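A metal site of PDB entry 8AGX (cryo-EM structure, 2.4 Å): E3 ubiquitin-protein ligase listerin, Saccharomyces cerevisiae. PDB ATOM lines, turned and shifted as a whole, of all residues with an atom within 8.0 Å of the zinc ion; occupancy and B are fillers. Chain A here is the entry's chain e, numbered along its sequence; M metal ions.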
ATOM      1  N   THR A1526      -5.332  32.462  23.862  1.00  0.00           N
ATOM      2  CA  THR A1526      -6.271  31.690  23.066  1.00  0.00           C
ATOM      3  C   THR A1526      -5.826  30.260  23.048  1.00  0.00           C
ATOM      4  O   THR A1526      -4.645  29.975  23.219  1.00  0.00           O
ATOM      5  CB  THR A1526      -6.347  32.160  21.610  1.00  0.00           C
ATOM      6  OG1 THR A1526      -5.137  31.801  20.923  1.00  0.00           O
ATOM      7  CG2 THR A1526      -6.539  33.661  21.519  1.00  0.00           C
ATOM      8  N   CYS A1527      -6.758  29.343  22.814  1.00  0.00           N
ATOM      9  CA  CYS A1527      -6.419  27.936  22.865  1.00  0.00           C
ATOM     10  C   CYS A1527      -5.979  27.393  21.528  1.00  0.00           C
ATOM     11  O   CYS A1527      -6.615  27.641  20.515  1.00  0.00           O
ATOM     12  CB  CYS A1527      -7.600  27.153  23.377  1.00  0.00           C
ATOM     13  SG  CYS A1527      -7.451  25.378  23.231  1.00  0.00           S
ATOM     14  N   PRO A1528      -4.877  26.650  21.512  1.00  0.00           N
ATOM     15  CA  PRO A1528      -4.536  26.087  20.225  1.00  0.00           C
ATOM     16  C   PRO A1528      -5.584  25.130  19.731  1.00  0.00           C
ATOM     17  O   PRO A1528      -5.947  25.179  18.562  1.00  0.00           O
ATOM     18  CB  PRO A1528      -3.268  25.309  20.538  1.00  0.00           C
ATOM     19  CG  PRO A1528      -2.641  26.037  21.669  1.00  0.00           C
ATOM     20  CD  PRO A1528      -3.795  26.516  22.495  1.00  0.00           C
ATOM     21  N   THR A1529      -6.078  24.271  20.601  1.00  0.00           N
ATOM     22  CA  THR A1529      -7.044  23.258  20.185  1.00  0.00           C
ATOM     23  C   THR A1529      -8.362  23.826  19.694  1.00  0.00           C
ATOM     24  O   THR A1529      -8.905  23.351  18.699  1.00  0.00           O
ATOM     25  CB  THR A1529      -7.337  22.303  21.349  1.00  0.00           C
ATOM     26  OG1 THR A1529      -6.099  21.955  21.988  1.00  0.00           O
ATOM     27  CG2 THR A1529      -8.019  21.044  20.842  1.00  0.00           C
ATOM     28  N   CYS A1530      -8.887  24.830  20.373  1.00  0.00           N
ATOM     29  CA  CYS A1530     -10.191  25.379  19.997  1.00  0.00           C
ATOM     30  C   CYS A1530     -10.191  26.883  20.191  1.00  0.00           C
ATOM     31  O   CYS A1530      -9.306  27.425  20.824  1.00  0.00           O
ATOM     32  CB  CYS A1530     -11.315  24.736  20.804  1.00  0.00           C
ATOM     33  SG  CYS A1530     -11.484  25.318  22.497  1.00  0.00           S
ATOM     34  N   LYS A1531     -11.165  27.588  19.639  1.00  0.00           N
ATOM     35  CA  LYS A1531     -11.145  29.027  19.736  1.00  0.00           C
ATOM     36  C   LYS A1531     -11.734  29.490  21.049  1.00  0.00           C
ATOM     37  O   LYS A1531     -12.866  29.969  21.095  1.00  0.00           O
ATOM     38  CB  LYS A1531     -11.926  29.644  18.579  1.00  0.00           C
ATOM     39  CG  LYS A1531     -11.883  28.865  17.274  1.00  0.00           C
ATOM     40  CD  LYS A1531     -13.143  28.030  17.090  1.00  0.00           C
ATOM     41  CE  LYS A1531     -12.968  27.014  15.987  1.00  0.00           C
ATOM     42  NZ  LYS A1531     -14.157  26.126  15.875  1.00  0.00           N
ATOM     43  N   ASN A1532     -10.968  29.357  22.123  1.00  0.00           N
ATOM     44  CA  ASN A1532     -11.448  29.787  23.418  1.00  0.00           C
ATOM     45  C   ASN A1532     -10.526  30.872  23.918  1.00  0.00           C
ATOM     46  O   ASN A1532      -9.317  30.723  23.832  1.00  0.00           O
ATOM     47  CB  ASN A1532     -11.534  28.601  24.348  1.00  0.00           C
ATOM     48  CG  ASN A1532     -12.931  28.039  24.441  1.00  0.00           C
ATOM     49  OD1 ASN A1532     -13.118  26.888  24.821  1.00  0.00           O
ATOM     50  ND2 ASN A1532     -13.907  28.854  24.083  1.00  0.00           N
ATOM     51  N   LYS A1533     -11.071  31.972  24.422  1.00  0.00           N
ATOM     52  CA  LYS A1533     -10.216  33.102  24.808  1.00  0.00           C
ATOM     53  C   LYS A1533     -10.185  33.359  26.280  1.00  0.00           C
ATOM     54  O   LYS A1533     -11.231  33.478  26.897  1.00  0.00           O
ATOM     55  CB  LYS A1533     -10.649  34.368  24.091  1.00  0.00           C
ATOM     56  CG  LYS A1533      -9.939  34.586  22.770  1.00  0.00           C
ATOM     57  CD  LYS A1533     -10.173  35.990  22.243  1.00  0.00           C
ATOM     58  CE  LYS A1533      -9.414  36.216  20.943  1.00  0.00           C
ATOM     59  NZ  LYS A1533      -9.679  37.556  20.363  1.00  0.00           N
ATOM     60  N   PHE A1534      -8.991  33.493  26.859  1.00  0.00           N
ATOM     61  CA  PHE A1534      -8.866  33.630  28.296  1.00  0.00           C
ATOM     62  C   PHE A1534      -8.014  34.794  28.705  1.00  0.00           C
ATOM     63  O   PHE A1534      -7.098  35.158  27.986  1.00  0.00           O
ATOM     64  CB  PHE A1534      -8.193  32.401  28.897  1.00  0.00           C
ATOM     65  CG  PHE A1534      -8.755  31.094  28.449  1.00  0.00           C
ATOM     66  CD1 PHE A1534      -9.829  30.526  29.097  1.00  0.00           C
ATOM     67  CD2 PHE A1534      -8.181  30.414  27.388  1.00  0.00           C
ATOM     68  CE1 PHE A1534     -10.339  29.312  28.691  1.00  0.00           C
ATOM     69  CE2 PHE A1534      -8.687  29.197  26.973  1.00  0.00           C
ATOM     70  CZ  PHE A1534      -9.764  28.648  27.637  1.00  0.00           C
ATOM     71  N   THR A1550      -3.589  22.971  30.361  1.00  0.00           N
ATOM     72  CA  THR A1550      -4.822  22.436  29.792  1.00  0.00           C
ATOM     73  C   THR A1550      -5.902  23.510  29.583  1.00  0.00           C
ATOM     74  O   THR A1550      -6.131  24.314  30.484  1.00  0.00           O
ATOM     75  CB  THR A1550      -5.395  21.300  30.638  1.00  0.00           C
ATOM     76  OG1 THR A1550      -5.351  21.676  32.023  1.00  0.00           O
ATOM     77  CG2 THR A1550      -4.595  20.026  30.443  1.00  0.00           C
ATOM     78  N   CYS A1551      -6.552  23.532  28.424  1.00  0.00           N
ATOM     79  CA  CYS A1551      -7.644  24.480  28.190  1.00  0.00           C
ATOM     80  C   CYS A1551      -8.657  24.015  29.202  1.00  0.00           C
ATOM     81  O   CYS A1551      -8.904  22.842  29.377  1.00  0.00           O
ATOM     82  CB  CYS A1551      -8.109  24.299  26.732  1.00  0.00           C
ATOM     83  SG  CYS A1551      -9.525  25.147  25.997  1.00  0.00           S
ATOM     84  N   PRO A1552      -9.179  24.942  29.986  1.00  0.00           N
ATOM     85  CA  PRO A1552     -10.106  24.374  30.954  1.00  0.00           C
ATOM     86  C   PRO A1552     -11.350  23.823  30.293  1.00  0.00           C
ATOM     87  O   PRO A1552     -11.768  22.711  30.598  1.00  0.00           O
ATOM     88  CB  PRO A1552     -10.417  25.530  31.906  1.00  0.00           C
ATOM     89  CG  PRO A1552      -9.279  26.485  31.723  1.00  0.00           C
ATOM     90  CD  PRO A1552      -8.833  26.334  30.295  1.00  0.00           C
ATOM     91  N   LEU A1553     -11.929  24.569  29.375  1.00  0.00           N
ATOM     92  CA  LEU A1553     -13.146  24.113  28.756  1.00  0.00           C
ATOM     93  C   LEU A1553     -12.946  22.861  27.929  1.00  0.00           C
ATOM     94  O   LEU A1553     -13.739  21.934  28.026  1.00  0.00           O
ATOM     95  CB  LEU A1553     -13.755  25.227  27.921  1.00  0.00           C
ATOM     96  CG  LEU A1553     -14.300  26.417  28.696  1.00  0.00           C
ATOM     97  CD1 LEU A1553     -15.247  27.170  27.787  1.00  0.00           C
ATOM     98  CD2 LEU A1553     -15.031  25.947  29.945  1.00  0.00           C
ATOM     99  N   CYS A1554     -11.876  22.802  27.145  1.00  0.00           N
ATOM    100  CA  CYS A1554     -11.581  21.590  26.408  1.00  0.00           C
ATOM    101  C   CYS A1554     -10.385  21.002  27.111  1.00  0.00           C
ATOM    102  O   CYS A1554      -9.371  21.627  27.173  1.00  0.00           O
ATOM    103  CB  CYS A1554     -11.352  21.858  24.903  1.00  0.00           C
ATOM    104  SG  CYS A1554      -9.726  22.343  24.264  1.00  0.00           S
ATOM    105  N   ARG A1555     -10.437  19.750  27.527  1.00  0.00           N
ATOM    106  CA  ARG A1555      -9.347  19.216  28.358  1.00  0.00           C
ATOM    107  C   ARG A1555      -8.002  19.227  27.682  1.00  0.00           C
ATOM    108  O   ARG A1555      -6.982  19.092  28.339  1.00  0.00           O
ATOM    109  CB  ARG A1555      -9.696  17.819  28.849  1.00  0.00           C
ATOM    110  CG  ARG A1555     -10.076  17.757  30.325  1.00  0.00           C
ATOM    111  CD  ARG A1555     -11.220  18.706  30.638  1.00  0.00           C
ATOM    112  NE  ARG A1555     -11.446  18.849  32.068  1.00  0.00           N
ATOM    113  CZ  ARG A1555     -10.876  19.774  32.828  1.00  0.00           C
ATOM    114  NH1 ARG A1555     -10.046  20.658  32.281  1.00  0.00           N
ATOM    115  NH2 ARG A1555     -11.132  19.833  34.121  1.00  0.00           N
ATOM    116  N   SER A1556      -7.984  19.374  26.366  1.00  0.00           N
ATOM    117  CA  SER A1556      -6.746  19.343  25.607  1.00  0.00           C
ATOM    118  C   SER A1556      -5.715  20.360  25.995  1.00  0.00           C
ATOM    119  O   SER A1556      -6.045  21.477  26.389  1.00  0.00           O
ATOM    120  CB  SER A1556      -7.064  19.524  24.133  1.00  0.00           C
ATOM    121  OG  SER A1556      -5.874  19.500  23.361  1.00  0.00           O
ATOM    122  N   GLU A1557      -4.447  19.991  25.877  1.00  0.00           N
ATOM    123  CA  GLU A1557      -3.352  20.868  26.291  1.00  0.00           C
ATOM    124  C   GLU A1557      -3.085  22.157  25.519  1.00  0.00           C
ATOM    125  O   GLU A1557      -3.308  22.230  24.317  1.00  0.00           O
ATOM    126  CB  GLU A1557      -2.053  20.060  26.352  1.00  0.00           C
ATOM    127  N   ILE A1558      -2.626  23.188  26.229  1.00  0.00           N
ATOM    128  CA  ILE A1558      -2.296  24.461  25.606  1.00  0.00           C
ATOM    129  C   ILE A1558      -0.821  24.667  25.815  1.00  0.00           C
ATOM    130  O   ILE A1558      -0.326  24.526  26.925  1.00  0.00           O
ATOM    131  CB  ILE A1558      -3.009  25.617  26.323  1.00  0.00           C
ATOM    132  CG1 ILE A1558      -4.515  25.566  26.066  1.00  0.00           C
ATOM    133  CG2 ILE A1558      -2.459  26.968  25.895  1.00  0.00           C
ATOM    134  CD1 ILE A1558      -5.234  26.817  26.523  1.00  0.00           C
HETATM  135 ZN    ZN M   1      -9.603  24.619  23.680  1.00  0.00          ZN
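SG of Cys 1527 lies close to N of Thr 1529, 3.2 Å away. The backbone carbonyl oxygen (O) of Asn 1532 sits at hydrogen-bond distance from the backbone NH (N) of Cys 1527, 3.1 Å away. SG of Cys 1530 sits close to OD1 of Asn 1532, 3.2 Å away. The backbone carbonyl oxygen (O) of Ser 1556 lies within hydrogen-bond range of the backbone NH (N) of Cys 1551 (2.9 Å). OG1 of Thr 1529 lies within hydrogen-bond range of OG of Ser 1556, at 2.8 Å.
Residues that only touch the zinc ion: Thr 1529 (3.99 Å). Five residues have an atom within 4 Å of the zinc ion: Cys 1527, Thr 1529, Cys 1530, Cys 1551 and Cys 1554. Along chain A the residues within 4 Å of the zinc ion span positions 1527 to 1554.
The zinc ion is bound by SG of Cys 1527, SG of Cys 1530, SG of Cys 1554 and SG of Cys 1551. The zinc ion has four donor atoms within binding distance.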
